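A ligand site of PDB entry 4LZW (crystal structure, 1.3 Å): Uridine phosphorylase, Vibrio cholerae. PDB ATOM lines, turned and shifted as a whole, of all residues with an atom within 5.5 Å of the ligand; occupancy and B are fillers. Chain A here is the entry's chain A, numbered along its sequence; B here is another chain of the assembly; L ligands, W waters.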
ATOM      1  N   GLY A  67      -7.208 -37.403 -11.099  1.00  0.00           N
ATOM      2  CA  GLY A  67      -6.466 -37.044  -9.914  1.00  0.00           C
ATOM      3  C   GLY A  67      -5.386 -36.051 -10.278  1.00  0.00           C
ATOM      4  O   GLY A  67      -5.198 -35.733 -11.454  1.00  0.00           O
ATOM      5  N   ILE A  68      -4.672 -35.572  -9.280  1.00  0.00           N
ATOM      6  CA  ILE A  68      -3.563 -34.671  -9.543  1.00  0.00           C
ATOM      7  C   ILE A  68      -2.318 -35.471  -9.853  1.00  0.00           C
ATOM      8  O   ILE A  68      -1.969 -36.402  -9.132  1.00  0.00           O
ATOM      9  CB  ILE A  68      -3.312 -33.781  -8.320  1.00  0.00           C
ATOM     10  CG1 ILE A  68      -4.486 -32.832  -8.118  1.00  0.00           C
ATOM     11  CG2 ILE A  68      -1.985 -33.060  -8.456  1.00  0.00           C
ATOM     12  CD1 ILE A  68      -4.371 -32.058  -6.822  1.00  0.00           C
ATOM     13  N   GLY A  69      -1.625 -35.074 -10.908  1.00  0.00           N
ATOM     14  CA  GLY A  69      -0.307 -35.596 -11.190  1.00  0.00           C
ATOM     15  C   GLY A  69      -0.244 -36.653 -12.265  1.00  0.00           C
ATOM     16  O   GLY A  69      -1.217 -37.346 -12.572  1.00  0.00           O
ATOM     17  N   ARG A  90      -7.515 -33.151 -22.174  1.00  0.00           N
ATOM     18  CA  ARG A  90      -7.251 -32.704 -20.824  1.00  0.00           C
ATOM     19  C   ARG A  90      -7.763 -31.280 -20.636  1.00  0.00           C
ATOM     20  O   ARG A  90      -7.504 -30.411 -21.462  1.00  0.00           O
ATOM     21  CB  ARG A  90      -5.753 -32.740 -20.588  1.00  0.00           C
ATOM     22  CG  ARG A  90      -5.328 -32.048 -19.331  1.00  0.00           C
ATOM     23  CD  ARG A  90      -5.756 -32.872 -18.195  1.00  0.00           C
ATOM     24  NE  ARG A  90      -5.299 -32.322 -16.926  1.00  0.00           N
ATOM     25  CZ  ARG A  90      -5.628 -32.868 -15.772  1.00  0.00           C
ATOM     26  NH1 ARG A  90      -6.390 -33.942 -15.744  1.00  0.00           N
ATOM     27  NH2 ARG A  90      -5.188 -32.326 -14.650  1.00  0.00           N
ATOM     28  N   THR A  93      -7.150 -26.358 -14.408  1.00  0.00           N
ATOM     29  CA  THR A  93      -6.799 -25.009 -14.065  1.00  0.00           C
ATOM     30  C   THR A  93      -5.289 -24.881 -14.049  1.00  0.00           C
ATOM     31  O   THR A  93      -4.560 -25.874 -14.022  1.00  0.00           O
ATOM     32  CB  THR A  93      -7.290 -24.664 -12.647  1.00  0.00           C
ATOM     33  OG1 THR A  93      -6.710 -25.572 -11.714  1.00  0.00           O
ATOM     34  CG2 THR A  93      -8.801 -24.768 -12.593  1.00  0.00           C
ATOM     35  N   THR A  94      -4.809 -23.653 -14.080  1.00  0.00           N
ATOM     36  CA  THR A  94      -3.385 -23.462 -14.210  1.00  0.00           C
ATOM     37  C   THR A  94      -2.977 -22.129 -13.623  1.00  0.00           C
ATOM     38  O   THR A  94      -3.786 -21.208 -13.469  1.00  0.00           O
ATOM     39  CB  THR A  94      -2.970 -23.559 -15.696  1.00  0.00           C
ATOM     40  OG1 THR A  94      -1.557 -23.570 -15.789  1.00  0.00           O
ATOM     41  CG2 THR A  94      -3.458 -22.388 -16.500  1.00  0.00           C
ATOM     42  N   GLY A  95      -1.692 -22.018 -13.293  1.00  0.00           N
ATOM     43  CA  GLY A  95      -1.149 -20.737 -12.916  1.00  0.00           C
ATOM     44  C   GLY A  95      -0.311 -20.218 -14.060  1.00  0.00           C
ATOM     45  O   GLY A  95       0.578 -20.912 -14.542  1.00  0.00           O
ATOM     46  N   PHE A 161       3.213 -29.273  -6.805  1.00  0.00           N
ATOM     47  CA  PHE A 161       2.531 -27.994  -6.817  1.00  0.00           C
ATOM     48  C   PHE A 161       3.413 -26.924  -6.198  1.00  0.00           C
ATOM     49  O   PHE A 161       3.351 -25.756  -6.557  1.00  0.00           O
ATOM     50  CB  PHE A 161       1.244 -28.120  -6.004  1.00  0.00           C
ATOM     51  CG  PHE A 161       0.393 -26.902  -6.037  1.00  0.00           C
ATOM     52  CD1 PHE A 161      -0.475 -26.702  -7.090  1.00  0.00           C
ATOM     53  CD2 PHE A 161       0.420 -25.963  -5.017  1.00  0.00           C
ATOM     54  CE1 PHE A 161      -1.284 -25.600  -7.144  1.00  0.00           C
ATOM     55  CE2 PHE A 161      -0.383 -24.849  -5.052  1.00  0.00           C
ATOM     56  CZ  PHE A 161      -1.239 -24.666  -6.117  1.00  0.00           C
ATOM     57  N   GLN A 165       7.002 -25.631  -8.727  1.00  0.00           N
ATOM     58  CA  GLN A 165       6.437 -24.412  -9.301  1.00  0.00           C
ATOM     59  C   GLN A 165       7.014 -23.223  -8.554  1.00  0.00           C
ATOM     60  O   GLN A 165       6.471 -22.123  -8.593  1.00  0.00           O
ATOM     61  CB  GLN A 165       4.925 -24.440  -9.243  1.00  0.00           C
ATOM     62  CG  GLN A 165       4.426 -25.722  -9.898  1.00  0.00           C
ATOM     63  CD  GLN A 165       2.935 -25.768 -10.077  1.00  0.00           C
ATOM     64  OE1 GLN A 165       2.266 -24.743 -10.142  1.00  0.00           O
ATOM     65  NE2 GLN A 165       2.392 -26.968 -10.167  1.00  0.00           N
ATOM     66  N   ARG A 167       7.171 -22.291  -5.454  1.00  0.00           N
ATOM     67  CA  ARG A 167       6.466 -21.635  -4.387  1.00  0.00           C
ATOM     68  C   ARG A 167       7.298 -21.650  -3.125  1.00  0.00           C
ATOM     69  O   ARG A 167       7.928 -22.661  -2.810  1.00  0.00           O
ATOM     70  CB  ARG A 167       5.154 -22.365  -4.137  1.00  0.00           C
ATOM     71  CG  ARG A 167       4.116 -22.056  -5.194  1.00  0.00           C
ATOM     72  CD  ARG A 167       2.816 -22.770  -4.883  1.00  0.00           C
ATOM     73  NE  ARG A 167       1.718 -22.141  -5.609  1.00  0.00           N
ATOM     74  CZ  ARG A 167       1.276 -22.504  -6.809  1.00  0.00           C
ATOM     75  NH1 ARG A 167       1.804 -23.547  -7.435  1.00  0.00           N
ATOM     76  NH2 ARG A 167       0.290 -21.819  -7.366  1.00  0.00           N
ATOM     77  N   PHE A 194       2.091 -23.123 -15.403  1.00  0.00           N
ATOM     78  CA  PHE A 194       2.383 -24.355 -14.685  1.00  0.00           C
ATOM     79  C   PHE A 194       1.122 -25.186 -14.517  1.00  0.00           C
ATOM     80  O   PHE A 194       0.063 -24.688 -14.146  1.00  0.00           O
ATOM     81  CB  PHE A 194       2.807 -24.032 -13.244  1.00  0.00           C
ATOM     82  CG  PHE A 194       4.232 -23.606 -13.064  1.00  0.00           C
ATOM     83  CD1 PHE A 194       5.284 -24.466 -13.337  1.00  0.00           C
ATOM     84  CD2 PHE A 194       4.501 -22.365 -12.507  1.00  0.00           C
ATOM     85  CE1 PHE A 194       6.586 -24.071 -13.106  1.00  0.00           C
ATOM     86  CE2 PHE A 194       5.803 -21.979 -12.255  1.00  0.00           C
ATOM     87  CZ  PHE A 194       6.841 -22.822 -12.564  1.00  0.00           C
ATOM     88  N   GLU A 195       1.244 -26.494 -14.747  1.00  0.00           N
ATOM     89  CA  GLU A 195       0.281 -27.428 -14.221  1.00  0.00           C
ATOM     90  C   GLU A 195       1.035 -28.722 -13.921  1.00  0.00           C
ATOM     91  O   GLU A 195       2.256 -28.668 -13.818  1.00  0.00           O
ATOM     92  CB  GLU A 195      -0.957 -27.585 -15.124  1.00  0.00           C
ATOM     93  CG  GLU A 195      -0.653 -27.825 -16.559  1.00  0.00           C
ATOM     94  CD  GLU A 195      -0.153 -29.221 -16.780  1.00  0.00           C
ATOM     95  OE1 GLU A 195       1.064 -29.379 -16.942  1.00  0.00           O
ATOM     96  OE2 GLU A 195      -0.976 -30.142 -16.739  1.00  0.00           O
ATOM     97  N   MET A 196       0.346 -29.852 -13.764  1.00  0.00           N
ATOM     98  CA  MET A 196       0.997 -31.023 -13.171  1.00  0.00           C
ATOM     99  C   MET A 196       0.800 -32.324 -13.930  1.00  0.00           C
ATOM    100  O   MET A 196       1.240 -33.370 -13.468  1.00  0.00           O
ATOM    101  CB  MET A 196       0.539 -31.208 -11.733  1.00  0.00           C
ATOM    102  CG  MET A 196       0.990 -30.045 -10.897  1.00  0.00           C
ATOM    103  SD  MET A 196       0.517 -30.210  -9.181  1.00  0.00           S
ATOM    104  CE  MET A 196       1.486 -31.644  -8.693  1.00  0.00           C
ATOM    105  N   GLU A 197       0.121 -32.277 -15.080  1.00  0.00           N
ATOM    106  CA  GLU A 197      -0.257 -33.513 -15.746  1.00  0.00           C
ATOM    107  C   GLU A 197       0.095 -33.575 -17.218  1.00  0.00           C
ATOM    108  O   GLU A 197       0.170 -34.665 -17.779  1.00  0.00           O
ATOM    109  CB  GLU A 197      -1.759 -33.730 -15.610  1.00  0.00           C
ATOM    110  CG  GLU A 197      -2.206 -33.943 -14.164  1.00  0.00           C
ATOM    111  CD  GLU A 197      -2.333 -32.662 -13.354  1.00  0.00           C
ATOM    112  OE1 GLU A 197      -2.346 -31.543 -13.934  1.00  0.00           O
ATOM    113  OE2 GLU A 197      -2.423 -32.771 -12.127  1.00  0.00           O
ATOM    114  N   ILE A 219      -6.177 -19.425 -13.485  1.00  0.00           N
ATOM    115  CA  ILE A 219      -6.892 -18.938 -12.307  1.00  0.00           C
ATOM    116  C   ILE A 219      -6.007 -18.125 -11.386  1.00  0.00           C
ATOM    117  O   ILE A 219      -6.489 -17.548 -10.418  1.00  0.00           O
ATOM    118  CB  ILE A 219      -7.600 -20.063 -11.541  1.00  0.00           C
ATOM    119  CG1 ILE A 219      -6.583 -21.033 -10.944  1.00  0.00           C
ATOM    120  CG2 ILE A 219      -8.599 -20.757 -12.457  1.00  0.00           C
ATOM    121  CD1 ILE A 219      -7.173 -22.014  -9.960  1.00  0.00           C
ATOM    122  N   ILE A 220      -4.719 -18.080 -11.697  1.00  0.00           N
ATOM    123  CA  ILE A 220      -3.825 -17.233 -10.952  1.00  0.00           C
ATOM    124  C   ILE A 220      -2.714 -16.857 -11.888  1.00  0.00           C
ATOM    125  O   ILE A 220      -2.339 -17.616 -12.793  1.00  0.00           O
ATOM    126  CB  ILE A 220      -3.229 -17.956  -9.697  1.00  0.00           C
ATOM    127  CG1 ILE A 220      -2.271 -17.049  -8.928  1.00  0.00           C
ATOM    128  CG2 ILE A 220      -2.514 -19.234 -10.090  1.00  0.00           C
ATOM    129  CD1 ILE A 220      -1.889 -17.636  -7.584  1.00  0.00           C
ATOM    130  N   ARG A 222       1.150 -16.046 -11.482  1.00  0.00           N
ATOM    131  CA  ARG A 222       2.230 -16.181 -10.527  1.00  0.00           C
ATOM    132  C   ARG A 222       3.158 -14.989 -10.465  1.00  0.00           C
ATOM    133  O   ARG A 222       3.992 -14.913  -9.579  1.00  0.00           O
ATOM    134  CB  ARG A 222       3.011 -17.450 -10.832  1.00  0.00           C
ATOM    135  CG  ARG A 222       2.234 -18.725 -10.526  1.00  0.00           C
ATOM    136  CD  ARG A 222       2.015 -18.923  -9.019  1.00  0.00           C
ATOM    137  NE  ARG A 222       3.277 -18.798  -8.296  1.00  0.00           N
ATOM    138  CZ  ARG A 222       4.194 -19.760  -8.260  1.00  0.00           C
ATOM    139  NH1 ARG A 222       5.333 -19.555  -7.613  1.00  0.00           N
ATOM    140  NH2 ARG A 222       3.990 -20.932  -8.864  1.00  0.00           N
ATOM    141  N   GLU A 226       1.296 -16.240  -5.095  1.00  0.00           N
ATOM    142  CA  GLU A 226       1.561 -17.675  -5.172  1.00  0.00           C
ATOM    143  C   GLU A 226       0.337 -18.556  -5.148  1.00  0.00           C
ATOM    144  O   GLU A 226       0.318 -19.579  -5.808  1.00  0.00           O
ATOM    145  CB  GLU A 226       2.442 -18.132  -4.017  1.00  0.00           C
ATOM    146  CG  GLU A 226       3.859 -17.733  -4.143  1.00  0.00           C
ATOM    147  CD  GLU A 226       4.796 -18.522  -3.242  1.00  0.00           C
ATOM    148  OE1 GLU A 226       4.343 -19.392  -2.465  1.00  0.00           O
ATOM    149  OE2 GLU A 226       6.003 -18.254  -3.319  1.00  0.00           O
ATOM    150  N   PRO A 228      -3.972 -19.302  -5.222  1.00  0.00           N
ATOM    151  CA  PRO A 228      -5.294 -18.750  -5.524  1.00  0.00           C
ATOM    152  C   PRO A 228      -6.163 -18.730  -4.274  1.00  0.00           C
ATOM    153  O   PRO A 228      -6.010 -19.624  -3.443  1.00  0.00           O
ATOM    154  CB  PRO A 228      -5.867 -19.755  -6.537  1.00  0.00           C
ATOM    155  CG  PRO A 228      -4.731 -20.633  -6.938  1.00  0.00           C
ATOM    156  CD  PRO A 228      -3.797 -20.647  -5.776  1.00  0.00           C
ATOM    157  N   PHE B   6      -4.971 -24.863   0.399  1.00  0.00           N
ATOM    158  CA  PHE B   6      -5.614 -24.757  -0.891  1.00  0.00           C
ATOM    159  C   PHE B   6      -6.280 -26.024  -1.367  1.00  0.00           C
ATOM    160  O   PHE B   6      -7.382 -25.986  -1.876  1.00  0.00           O
ATOM    161  CB  PHE B   6      -4.604 -24.294  -1.924  1.00  0.00           C
ATOM    162  CG  PHE B   6      -5.191 -24.099  -3.280  1.00  0.00           C
ATOM    163  CD1 PHE B   6      -6.169 -23.133  -3.482  1.00  0.00           C
ATOM    164  CD2 PHE B   6      -4.771 -24.868  -4.345  1.00  0.00           C
ATOM    165  CE1 PHE B   6      -6.714 -22.945  -4.733  1.00  0.00           C
ATOM    166  CE2 PHE B   6      -5.313 -24.694  -5.588  1.00  0.00           C
ATOM    167  CZ  PHE B   6      -6.290 -23.720  -5.786  1.00  0.00           C
ATOM    168  N   HIS B   7      -5.584 -27.151  -1.229  1.00  0.00           N
ATOM    169  CA  HIS B   7      -6.149 -28.403  -1.715  1.00  0.00           C
ATOM    170  C   HIS B   7      -6.930 -29.147  -0.674  1.00  0.00           C
ATOM    171  O   HIS B   7      -8.012 -29.624  -0.947  1.00  0.00           O
ATOM    172  CB  HIS B   7      -5.063 -29.313  -2.254  1.00  0.00           C
ATOM    173  CG  HIS B   7      -4.381 -28.770  -3.464  1.00  0.00           C
ATOM    174  ND1 HIS B   7      -3.262 -27.977  -3.388  1.00  0.00           N
ATOM    175  CD2 HIS B   7      -4.690 -28.865  -4.777  1.00  0.00           C
ATOM    176  CE1 HIS B   7      -2.880 -27.640  -4.605  1.00  0.00           C
ATOM    177  NE2 HIS B   7      -3.734 -28.155  -5.466  1.00  0.00           N
ATOM    178  N   ARG B  47     -11.225 -33.347  -4.131  1.00  0.00           N
ATOM    179  CA  ARG B  47     -10.399 -34.137  -5.025  1.00  0.00           C
ATOM    180  C   ARG B  47     -10.097 -35.490  -4.360  1.00  0.00           C
ATOM    181  O   ARG B  47     -10.982 -36.102  -3.763  1.00  0.00           O
ATOM    182  CB  ARG B  47      -9.142 -33.358  -5.397  1.00  0.00           C
ATOM    183  CG  ARG B  47      -9.437 -32.093  -6.188  1.00  0.00           C
ATOM    184  CD  ARG B  47      -8.162 -31.328  -6.459  1.00  0.00           C
ATOM    185  NE  ARG B  47      -8.330 -30.215  -7.383  1.00  0.00           N
ATOM    186  CZ  ARG B  47      -8.074 -30.275  -8.691  1.00  0.00           C
ATOM    187  NH1 ARG B  47      -7.647 -31.394  -9.246  1.00  0.00           N
ATOM    188  NH2 ARG B  47      -8.252 -29.204  -9.444  1.00  0.00           N
ATOM    189  N   ILE B  75       1.428 -32.823  -2.194  1.00  0.00           N
ATOM    190  CA  ILE B  75       0.536 -31.730  -1.839  1.00  0.00           C
ATOM    191  C   ILE B  75      -0.032 -31.971  -0.447  1.00  0.00           C
ATOM    192  O   ILE B  75      -0.082 -31.056   0.374  1.00  0.00           O
ATOM    193  CB  ILE B  75      -0.610 -31.621  -2.866  1.00  0.00           C
ATOM    194  CG1 ILE B  75      -0.061 -31.037  -4.159  1.00  0.00           C
ATOM    195  CG2 ILE B  75      -1.771 -30.828  -2.317  1.00  0.00           C
ATOM    196  CD1 ILE B  75      -1.022 -31.127  -5.304  1.00  0.00           C
HETATM  197  O1  LIG L   1      -3.668 -27.636  -8.170  1.00  0.00           O
HETATM  198  C1  LIG L   1      -4.717 -28.266  -8.750  1.00  0.00           C
HETATM  199  C2  LIG L   1      -4.623 -28.679 -10.140  1.00  0.00           C
HETATM  200  O2  LIG L   1      -4.344 -27.568 -10.946  1.00  0.00           O
HETATM  201  C3  LIG L   1      -3.498 -29.627 -10.357  1.00  0.00           C
HETATM  202  O3  LIG L   1      -3.829 -30.454 -11.383  1.00  0.00           O
HETATM  203  C4  LIG L   1      -2.371 -28.756 -10.706  1.00  0.00           C
HETATM  204  C5  LIG L   1      -2.953 -27.523 -11.308  1.00  0.00           C
HETATM  205  N1  LIG L   1      -2.395 -26.232 -10.908  1.00  0.00           N
HETATM  206  C6  LIG L   1      -1.038 -26.052 -10.897  1.00  0.00           C
HETATM  207  O4  LIG L   1      -0.287 -26.951 -11.160  1.00  0.00           O
HETATM  208  N2  LIG L   1      -0.532 -24.872 -10.532  1.00  0.00           N
HETATM  209  C7  LIG L   1      -1.313 -23.833 -10.208  1.00  0.00           C
HETATM  210  O5  LIG L   1      -0.718 -22.704  -9.873  1.00  0.00           O
HETATM  211  C8  LIG L   1      -2.710 -23.963 -10.221  1.00  0.00           C
HETATM  212  C9  LIG L   1      -3.593 -22.779  -9.850  1.00  0.00           C
HETATM  213  C10 LIG L   1      -3.233 -25.222 -10.602  1.00  0.00           C
HETATM  214  O   HOH W   1      -5.536 -32.752 -11.862  1.00  0.00           O
HETATM  215  O   HOH W   2       1.891 -22.017 -10.488  1.00  0.00           O
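A ring nitrogen (NE2) of His 7 of chain B lies within hydrogen-bond range of an oxygen (O1) of the ligand.
The side-chain carboxylate (OE2) of Glu 197 is in hydrogen-bond range of an oxygen (O3) of the ligand (2.8 Å).
OE1 of Gln 165 is in hydrogen-bond range of N2 of the ligand (2.8 Å).
The guanidinium group (NH2) of Arg 167 lies within hydrogen-bond range of an oxygen (O5) of the ligand.
OG1 of Thr 93 lies within hydrogen-bond range of O2 of the ligand, 3.2 Å away.
The side-chain carboxylate (OE1) of Glu 197 lies within salt-bridge range of the guanidinium group (NH2) of Arg 90, 3.0 Å away.
OE2 of Glu 197 is in hydrogen-bond range of N of Gly 69 (2.7 Å).
OE1 of Gln 165 lies within hydrogen-bond range of NH1 of Arg 167, at 3.0 Å.
O of Gln 165 sits at hydrogen-bond distance from NH2 of Arg 222, at 2.8 Å.
The backbone carbonyl oxygen (O) of Phe 161 lies within hydrogen-bond range of the guanidinium group (NH1) of Arg 167.
O of Glu 226 lies within hydrogen-bond range of NH2 of Arg 167.
The backbone NH (N) of Phe 161 lies close to the side-chain sulfur (SD) of Met 196, 3.7 Å away.
O of Gly 95 is in hydrogen-bond range of N of Phe 194 (2.8 Å).
Thr 94 touches the ligand.
Gly 95 touches the ligand.
CE1 of Phe 161 touches O1 of the ligand, at 3.3 Å.
O of Phe 194 touches N2 of the ligand, 3.7 Å away.
Glu 195 touches the ligand (CA to O4, 3.1 Å).
Met 196 touches the ligand (CG to O4, 3.4 Å).
Ile 219 touches the ligand.
Ile 220 touches the ligand (CG2 to C9, 3.7 Å).
CG of Pro 228 touches C9 of the ligand, 3.8 Å away.
Arg 47 of chain B touches the ligand.
15 residues have an atom within 4 Å of the ligand: Thr 93, Thr 94, Gly 95, Phe 161, Gln 165, Arg 167, Phe 194, Glu 195, Met 196, Glu 197, Ile 219, Ile 220, Pro 228, His 7 of chain B and Arg 47 of chain B.
The nearest printed residue that does not touch the ligand is Arg 90 (4.003 Å).
Water W2 lies within hydrogen-bond range of O5 of the ligand (2.8 Å), OE1 of Gln 165 (2.8 Å), NH2 of Arg 222 (2.9 Å) and NH1 of Arg 167 (3.4 Å).
Water W1 lies within hydrogen-bond range of the guanidinium group of Arg 90 (2.8 Å), an oxygen (O3) of the ligand (2.9 Å), the backbone carbonyl oxygen of Gly 67 (3.0 Å) and the side-chain carboxylate of Glu 197 (3.1 Å).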
